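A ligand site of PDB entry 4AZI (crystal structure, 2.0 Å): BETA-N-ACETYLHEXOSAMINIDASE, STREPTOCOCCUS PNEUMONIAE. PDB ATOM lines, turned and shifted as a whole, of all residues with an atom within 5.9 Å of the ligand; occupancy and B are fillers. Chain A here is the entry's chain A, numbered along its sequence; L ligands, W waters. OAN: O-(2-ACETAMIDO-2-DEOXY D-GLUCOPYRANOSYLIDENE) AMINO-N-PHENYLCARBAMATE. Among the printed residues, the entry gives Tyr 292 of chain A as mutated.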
ATOM      1  N   ASP A  16     -31.320   7.458  19.863  1.00  0.00           N
ATOM      2  CA  ASP A  16     -31.991   6.190  20.143  1.00  0.00           C
ATOM      3  C   ASP A  16     -33.229   6.035  19.248  1.00  0.00           C
ATOM      4  O   ASP A  16     -34.354   6.280  19.672  1.00  0.00           O
ATOM      5  CB  ASP A  16     -32.346   6.133  21.656  1.00  0.00           C
ATOM      6  CG  ASP A  16     -32.940   4.784  22.100  1.00  0.00           C
ATOM      7  OD1 ASP A  16     -33.007   3.814  21.312  1.00  0.00           O
ATOM      8  OD2 ASP A  16     -33.341   4.710  23.281  1.00  0.00           O
ATOM      9  N   ARG A  19     -35.727   2.412  20.355  1.00  0.00           N
ATOM     10  CA  ARG A  19     -36.942   2.405  21.157  1.00  0.00           C
ATOM     11  C   ARG A  19     -38.053   3.219  20.494  1.00  0.00           C
ATOM     12  O   ARG A  19     -39.241   2.890  20.609  1.00  0.00           O
ATOM     13  CB  ARG A  19     -36.654   2.963  22.557  1.00  0.00           C
ATOM     14  CG  ARG A  19     -35.756   2.093  23.419  1.00  0.00           C
ATOM     15  CD  ARG A  19     -35.700   2.656  24.830  1.00  0.00           C
ATOM     16  NE  ARG A  19     -34.889   1.850  25.745  1.00  0.00           N
ATOM     17  CZ  ARG A  19     -33.631   2.113  26.081  1.00  0.00           C
ATOM     18  NH1 ARG A  19     -32.995   3.153  25.546  1.00  0.00           N
ATOM     19  NH2 ARG A  19     -32.994   1.337  26.947  1.00  0.00           N
ATOM     20  N   ASN A  48     -32.495  -1.452  19.399  1.00  0.00           N
ATOM     21  CA  ASN A  48     -32.312  -1.121  20.817  1.00  0.00           C
ATOM     22  C   ASN A  48     -33.682  -1.218  21.462  1.00  0.00           C
ATOM     23  O   ASN A  48     -34.488  -0.265  21.417  1.00  0.00           O
ATOM     24  CB  ASN A  48     -31.679   0.272  20.982  1.00  0.00           C
ATOM     25  CG  ASN A  48     -31.213   0.555  22.406  1.00  0.00           C
ATOM     26  OD1 ASN A  48     -30.420  -0.188  22.987  1.00  0.00           O
ATOM     27  ND2 ASN A  48     -31.697   1.660  22.961  1.00  0.00           N
ATOM     28  N   HIS A 120     -31.135  -5.664  25.285  1.00  0.00           N
ATOM     29  CA  HIS A 120     -31.847  -4.645  24.520  1.00  0.00           C
ATOM     30  C   HIS A 120     -32.362  -5.129  23.176  1.00  0.00           C
ATOM     31  O   HIS A 120     -32.250  -4.427  22.164  1.00  0.00           O
ATOM     32  CB  HIS A 120     -30.961  -3.409  24.363  1.00  0.00           C
ATOM     33  CG  HIS A 120     -30.701  -2.687  25.655  1.00  0.00           C
ATOM     34  ND1 HIS A 120     -31.654  -1.946  26.280  1.00  0.00           N
ATOM     35  CD2 HIS A 120     -29.559  -2.598  26.437  1.00  0.00           C
ATOM     36  CE1 HIS A 120     -31.125  -1.411  27.403  1.00  0.00           C
ATOM     37  NE2 HIS A 120     -29.849  -1.806  27.493  1.00  0.00           N
ATOM     38  N   ASP A 182     -24.550  -3.812  26.107  1.00  0.00           N
ATOM     39  CA  ASP A 182     -24.732  -3.214  27.430  1.00  0.00           C
ATOM     40  C   ASP A 182     -25.790  -3.944  28.247  1.00  0.00           C
ATOM     41  O   ASP A 182     -26.613  -4.664  27.700  1.00  0.00           O
ATOM     42  CB  ASP A 182     -25.091  -1.715  27.352  1.00  0.00           C
ATOM     43  CG  ASP A 182     -26.277  -1.432  26.435  1.00  0.00           C
ATOM     44  OD1 ASP A 182     -26.356  -2.036  25.334  1.00  0.00           O
ATOM     45  OD2 ASP A 182     -27.109  -0.578  26.799  1.00  0.00           O
ATOM     46  N   GLU A 183     -25.733  -3.757  29.563  1.00  0.00           N
ATOM     47  CA  GLU A 183     -26.795  -4.122  30.495  1.00  0.00           C
ATOM     48  C   GLU A 183     -27.477  -5.476  30.219  1.00  0.00           C
ATOM     49  O   GLU A 183     -28.699  -5.526  30.025  1.00  0.00           O
ATOM     50  CB  GLU A 183     -27.844  -3.020  30.536  1.00  0.00           C
ATOM     51  CG  GLU A 183     -27.335  -1.622  30.865  1.00  0.00           C
ATOM     52  CD  GLU A 183     -28.468  -0.610  30.810  1.00  0.00           C
ATOM     53  OE1 GLU A 183     -29.167  -0.566  29.788  1.00  0.00           O
ATOM     54  OE2 GLU A 183     -28.684   0.116  31.809  1.00  0.00           O
ATOM     55  N   ALA A 191     -30.602  -5.398  37.359  1.00  0.00           N
ATOM     56  CA  ALA A 191     -29.392  -4.736  36.871  1.00  0.00           C
ATOM     57  C   ALA A 191     -28.130  -5.284  37.514  1.00  0.00           C
ATOM     58  O   ALA A 191     -27.278  -4.523  37.961  1.00  0.00           O
ATOM     59  CB  ALA A 191     -29.493  -3.214  37.036  1.00  0.00           C
ATOM     60  N   PHE A 227     -20.432  -1.245  23.847  1.00  0.00           N
ATOM     61  CA  PHE A 227     -20.424  -0.538  25.126  1.00  0.00           C
ATOM     62  C   PHE A 227     -19.503  -1.257  26.092  1.00  0.00           C
ATOM     63  O   PHE A 227     -19.205  -2.435  25.922  1.00  0.00           O
ATOM     64  CB  PHE A 227     -21.833  -0.403  25.705  1.00  0.00           C
ATOM     65  CG  PHE A 227     -22.735   0.456  24.865  1.00  0.00           C
ATOM     66  CD1 PHE A 227     -22.442   1.803  24.653  1.00  0.00           C
ATOM     67  CD2 PHE A 227     -23.859  -0.095  24.271  1.00  0.00           C
ATOM     68  CE1 PHE A 227     -23.270   2.582  23.872  1.00  0.00           C
ATOM     69  CE2 PHE A 227     -24.686   0.685  23.490  1.00  0.00           C
ATOM     70  CZ  PHE A 227     -24.386   2.026  23.281  1.00  0.00           C
ATOM     71  N   ASP A 229     -19.673  -2.200  29.289  1.00  0.00           N
ATOM     72  CA  ASP A 229     -20.201  -3.029  30.402  1.00  0.00           C
ATOM     73  C   ASP A 229     -19.614  -4.443  30.500  1.00  0.00           C
ATOM     74  O   ASP A 229     -19.126  -4.849  31.558  1.00  0.00           O
ATOM     75  CB  ASP A 229     -21.735  -3.174  30.322  1.00  0.00           C
ATOM     76  CG  ASP A 229     -22.451  -1.856  30.168  1.00  0.00           C
ATOM     77  OD1 ASP A 229     -22.018  -1.009  29.361  1.00  0.00           O
ATOM     78  OD2 ASP A 229     -23.479  -1.679  30.844  1.00  0.00           O
ATOM     79  N   TRP A 250     -19.204   4.667  28.857  1.00  0.00           N
ATOM     80  CA  TRP A 250     -20.207   5.577  29.378  1.00  0.00           C
ATOM     81  C   TRP A 250     -20.229   5.690  30.889  1.00  0.00           C
ATOM     82  O   TRP A 250     -20.632   6.720  31.421  1.00  0.00           O
ATOM     83  CB  TRP A 250     -21.583   5.200  28.835  1.00  0.00           C
ATOM     84  CG  TRP A 250     -22.074   3.900  29.374  1.00  0.00           C
ATOM     85  CD1 TRP A 250     -21.740   2.619  28.933  1.00  0.00           C
ATOM     86  CD2 TRP A 250     -22.964   3.696  30.512  1.00  0.00           C
ATOM     87  NE1 TRP A 250     -22.368   1.665  29.690  1.00  0.00           N
ATOM     88  CE2 TRP A 250     -23.111   2.238  30.659  1.00  0.00           C
ATOM     89  CE3 TRP A 250     -23.625   4.536  31.391  1.00  0.00           C
ATOM     90  CZ2 TRP A 250     -23.903   1.687  31.652  1.00  0.00           C
ATOM     91  CZ3 TRP A 250     -24.422   3.963  32.384  1.00  0.00           C
ATOM     92  CH2 TRP A 250     -24.548   2.568  32.510  1.00  0.00           C
ATOM     93  N   TRP A 254     -22.556   1.325  38.913  1.00  0.00           N
ATOM     94  CA  TRP A 254     -23.330   1.778  40.032  1.00  0.00           C
ATOM     95  C   TRP A 254     -23.103   0.731  41.098  1.00  0.00           C
ATOM     96  O   TRP A 254     -22.476  -0.300  40.813  1.00  0.00           O
ATOM     97  CB  TRP A 254     -24.773   1.848  39.558  1.00  0.00           C
ATOM     98  CG  TRP A 254     -25.789   2.384  40.521  1.00  0.00           C
ATOM     99  CD1 TRP A 254     -26.985   1.788  40.902  1.00  0.00           C
ATOM    100  CD2 TRP A 254     -25.744   3.662  41.260  1.00  0.00           C
ATOM    101  NE1 TRP A 254     -27.674   2.570  41.800  1.00  0.00           N
ATOM    102  CE2 TRP A 254     -26.979   3.709  42.061  1.00  0.00           C
ATOM    103  CE3 TRP A 254     -24.848   4.722  41.343  1.00  0.00           C
ATOM    104  CZ2 TRP A 254     -27.280   4.779  42.897  1.00  0.00           C
ATOM    105  CZ3 TRP A 254     -25.162   5.800  42.195  1.00  0.00           C
ATOM    106  CH2 TRP A 254     -26.346   5.824  42.950  1.00  0.00           C
ATOM    107  N   TYR A 257     -22.648  -2.884  40.336  1.00  0.00           N
ATOM    108  CA  TYR A 257     -22.568  -3.076  38.890  1.00  0.00           C
ATOM    109  C   TYR A 257     -21.113  -2.739  38.616  1.00  0.00           C
ATOM    110  O   TYR A 257     -20.784  -1.620  38.220  1.00  0.00           O
ATOM    111  CB  TYR A 257     -23.545  -2.144  38.167  1.00  0.00           C
ATOM    112  CG  TYR A 257     -23.820  -2.474  36.705  1.00  0.00           C
ATOM    113  CD1 TYR A 257     -24.495  -3.645  36.349  1.00  0.00           C
ATOM    114  CD2 TYR A 257     -23.440  -1.601  35.693  1.00  0.00           C
ATOM    115  CE1 TYR A 257     -24.764  -3.929  35.018  1.00  0.00           C
ATOM    116  CE2 TYR A 257     -23.700  -1.878  34.353  1.00  0.00           C
ATOM    117  CZ  TYR A 257     -24.362  -3.050  34.032  1.00  0.00           C
ATOM    118  OH  TYR A 257     -24.618  -3.333  32.705  1.00  0.00           O
ATOM    119  N   TYR A 280     -25.863  12.370  28.890  1.00  0.00           N
ATOM    120  CA  TYR A 280     -27.107  11.661  28.521  1.00  0.00           C
ATOM    121  C   TYR A 280     -28.342  12.550  28.691  1.00  0.00           C
ATOM    122  O   TYR A 280     -28.435  13.296  29.658  1.00  0.00           O
ATOM    123  CB  TYR A 280     -27.285  10.407  29.398  1.00  0.00           C
ATOM    124  CG  TYR A 280     -26.515   9.171  28.985  1.00  0.00           C
ATOM    125  CD1 TYR A 280     -25.517   9.218  28.007  1.00  0.00           C
ATOM    126  CD2 TYR A 280     -26.773   7.934  29.589  1.00  0.00           C
ATOM    127  CE1 TYR A 280     -24.803   8.075  27.632  1.00  0.00           C
ATOM    128  CE2 TYR A 280     -26.070   6.798  29.221  1.00  0.00           C
ATOM    129  CZ  TYR A 280     -25.109   6.863  28.242  1.00  0.00           C
ATOM    130  OH  TYR A 280     -24.412   5.720  27.873  1.00  0.00           O
ATOM    131  N   ILE A 282     -32.673  11.844  28.345  1.00  0.00           N
ATOM    132  CA  ILE A 282     -33.845  11.005  28.040  1.00  0.00           C
ATOM    133  C   ILE A 282     -34.975  11.957  27.680  1.00  0.00           C
ATOM    134  O   ILE A 282     -35.301  12.860  28.455  1.00  0.00           O
ATOM    135  CB  ILE A 282     -34.253  10.120  29.254  1.00  0.00           C
ATOM    136  CG1 ILE A 282     -33.148   9.113  29.592  1.00  0.00           C
ATOM    137  CG2 ILE A 282     -35.567   9.404  28.992  1.00  0.00           C
ATOM    138  CD1 ILE A 282     -33.243   8.534  31.001  1.00  0.00           C
ATOM    139  N   TYR A 292     -30.383  11.955  34.079  1.00  0.00           N
ATOM    140  CA  TYR A 292     -30.367  12.238  32.649  1.00  0.00           C
ATOM    141  C   TYR A 292     -31.485  13.178  32.190  1.00  0.00           C
ATOM    142  O   TYR A 292     -32.058  13.010  31.109  1.00  0.00           O
ATOM    143  CB  TYR A 292     -30.376  10.926  31.840  1.00  0.00           C
ATOM    144  CG  TYR A 292     -29.375   9.882  32.342  1.00  0.00           C
ATOM    145  CD1 TYR A 292     -28.064  10.233  32.663  1.00  0.00           C
ATOM    146  CD2 TYR A 292     -29.745   8.544  32.449  1.00  0.00           C
ATOM    147  CE1 TYR A 292     -27.159   9.273  33.099  1.00  0.00           C
ATOM    148  CE2 TYR A 292     -28.834   7.578  32.897  1.00  0.00           C
ATOM    149  CZ  TYR A 292     -27.546   7.948  33.210  1.00  0.00           C
ATOM    150  OH  TYR A 292     -26.649   7.009  33.642  1.00  0.00           O
ATOM    151  N   TRP A 329     -31.478   9.497  24.513  1.00  0.00           N
ATOM    152  CA  TRP A 329     -32.134   8.199  24.717  1.00  0.00           C
ATOM    153  C   TRP A 329     -33.638   8.287  24.766  1.00  0.00           C
ATOM    154  O   TRP A 329     -34.204   9.332  25.066  1.00  0.00           O
ATOM    155  CB  TRP A 329     -31.602   7.506  25.961  1.00  0.00           C
ATOM    156  CG  TRP A 329     -30.100   7.259  25.960  1.00  0.00           C
ATOM    157  CD1 TRP A 329     -29.123   8.029  26.574  1.00  0.00           C
ATOM    158  CD2 TRP A 329     -29.368   6.142  25.327  1.00  0.00           C
ATOM    159  NE1 TRP A 329     -27.876   7.480  26.381  1.00  0.00           N
ATOM    160  CE2 TRP A 329     -27.949   6.356  25.628  1.00  0.00           C
ATOM    161  CE3 TRP A 329     -29.723   5.042  24.549  1.00  0.00           C
ATOM    162  CZ2 TRP A 329     -26.956   5.498  25.183  1.00  0.00           C
ATOM    163  CZ3 TRP A 329     -28.715   4.172  24.108  1.00  0.00           C
ATOM    164  CH2 TRP A 329     -27.366   4.389  24.422  1.00  0.00           C
ATOM    165  N   ALA A 330     -34.302   7.166  24.459  1.00  0.00           N
ATOM    166  CA  ALA A 330     -35.748   7.130  24.392  1.00  0.00           C
ATOM    167  C   ALA A 330     -36.427   6.179  25.374  1.00  0.00           C
ATOM    168  O   ALA A 330     -37.464   5.583  25.037  1.00  0.00           O
ATOM    169  CB  ALA A 330     -36.176   6.843  22.967  1.00  0.00           C
ATOM    170  N   ASP A 331     -35.882   6.047  26.583  1.00  0.00           N
ATOM    171  CA  ASP A 331     -36.400   5.116  27.616  1.00  0.00           C
ATOM    172  C   ASP A 331     -37.922   5.055  27.739  1.00  0.00           C
ATOM    173  O   ASP A 331     -38.503   3.985  27.896  1.00  0.00           O
ATOM    174  CB  ASP A 331     -35.777   5.418  28.987  1.00  0.00           C
ATOM    175  CG  ASP A 331     -34.257   5.247  29.003  1.00  0.00           C
ATOM    176  OD1 ASP A 331     -33.588   5.614  27.997  1.00  0.00           O
ATOM    177  OD2 ASP A 331     -33.733   4.752  30.016  1.00  0.00           O
HETATM  178  CAH OAN L   1     -25.171   2.020  27.307  1.00  0.00           C
HETATM  179  CAG OAN L   1     -26.356   2.753  27.954  1.00  0.00           C
HETATM  180  OAN OAN L   1     -26.300   3.949  28.164  1.00  0.00           O
HETATM  181  NAI OAN L   1     -27.404   1.980  28.258  1.00  0.00           N
HETATM  182  CAB OAN L   1     -28.656   2.474  28.871  1.00  0.00           C
HETATM  183  CAC OAN L   1     -29.580   3.028  27.787  1.00  0.00           C
HETATM  184  OAJ OAN L   1     -30.291   1.942  27.163  1.00  0.00           O
HETATM  185  CAD OAN L   1     -30.568   4.024  28.355  1.00  0.00           C
HETATM  186  OAK OAN L   1     -31.396   4.473  27.286  1.00  0.00           O
HETATM  187  CAE OAN L   1     -29.800   5.224  28.940  1.00  0.00           C
HETATM  188  CAF OAN L   1     -30.674   6.298  29.602  1.00  0.00           C
HETATM  189  OAM OAN L   1     -31.325   5.758  30.756  1.00  0.00           O
HETATM  190  OAL OAN L   1     -28.783   4.827  29.907  1.00  0.00           O
HETATM  191  CAA OAN L   1     -28.400   3.516  29.983  1.00  0.00           C
HETATM  192  NAY OAN L   1     -27.764   3.154  31.074  1.00  0.00           N
HETATM  193  OAQ OAN L   1     -27.573   4.125  32.009  1.00  0.00           O
HETATM  194  CAP OAN L   1     -27.547   3.669  33.292  1.00  0.00           C
HETATM  195  OAR OAN L   1     -27.311   4.449  34.218  1.00  0.00           O
HETATM  196  NAO OAN L   1     -27.794   2.365  33.480  1.00  0.00           N
HETATM  197  CAS OAN L   1     -27.765   1.724  34.659  1.00  0.00           C
HETATM  198  CAT OAN L   1     -27.001   0.567  34.756  1.00  0.00           C
HETATM  199  CAU OAN L   1     -26.942  -0.140  35.960  1.00  0.00           C
HETATM  200  CAV OAN L   1     -27.653   0.302  37.066  1.00  0.00           C
HETATM  201  CAW OAN L   1     -28.427   1.467  36.975  1.00  0.00           C
HETATM  202  CAX OAN L   1     -28.494   2.180  35.769  1.00  0.00           C
HETATM  203  O   HOH W   1     -30.416   4.206  32.942  1.00  0.00           O
HETATM  204  O   HOH W   2     -28.895   0.702  25.440  1.00  0.00           O
HETATM  205  O   HOH W   3     -29.544  -1.541  33.755  1.00  0.00           O
HETATM  206  O   HOH W   4     -28.743   5.478  36.495  1.00  0.00           O
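The side-chain carboxylate (OD1) of Asp 331 lies within hydrogen-bond range of an oxygen (OAK) of the ligand (2.6 Å). NAI of the ligand is in hydrogen-bond range of OD2 of Asp 182 (3.0 Å). The guanidinium group (NH1) of Arg 19 sits at hydrogen-bond distance from an oxygen (OAK) of the ligand (2.7 Å). The side-chain hydroxyl of Tyr 280 lies within hydrogen-bond range of an oxygen (OAN) of the ligand (2.6 Å). An oxygen (OAR) of the ligand sits at hydrogen-bond distance from the side-chain hydroxyl of Tyr 292, at 2.7 Å. OE2 of Glu 183 is in hydrogen-bond range of NAO of the ligand, 2.9 Å away.
N of Ile 282 sits at hydrogen-bond distance from O of Tyr 292 (3.1 Å). The indole nitrogen (NE1) of Trp 250 is in hydrogen-bond range of the side-chain carboxylate (OD1) of Asp 229 (2.7 Å). NE2 of His 120 sits at hydrogen-bond distance from OE1 of Glu 183. N of Arg 19 lies within hydrogen-bond range of O of Asn 48 (3.1 Å). The side-chain carboxylate (OD2) of Asp 182 is in hydrogen-bond range of a ring nitrogen (NE2) of His 120 (3.1 Å). The side-chain hydroxyl (OH) of Tyr 257 sits at hydrogen-bond distance from the side-chain carboxylate (OD2) of Asp 229 (2.7 Å). OH of Tyr 257 lies close to N of Glu 183, at 3.4 Å. The guanidinium group (NH1) of Arg 19 lies within salt-bridge range of the side-chain carboxylate (OD2) of Asp 16, 2.8 Å away.
Residues that only touch the ligand: His 120, Ala 191, Phe 227, Trp 250, Tyr 257, Ile 282 and Trp 329. Within 4 Å of the ligand: Arg 19, His 120, Asp 182, Glu 183, Ala 191, Phe 227, Trp 250, Tyr 257, Tyr 280, Ile 282, Tyr 292, Trp 329 and Asp 331. Along chain A the residues within 4 Å of the ligand span positions 19 to 331.
Water W2 lies within hydrogen-bond range of OAJ of the ligand (2.5 Å), OD2 of Asp 182 (2.6 Å), OD1 of Asn 48 (3.0 Å) and NE2 of His 120 (3.4 Å).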
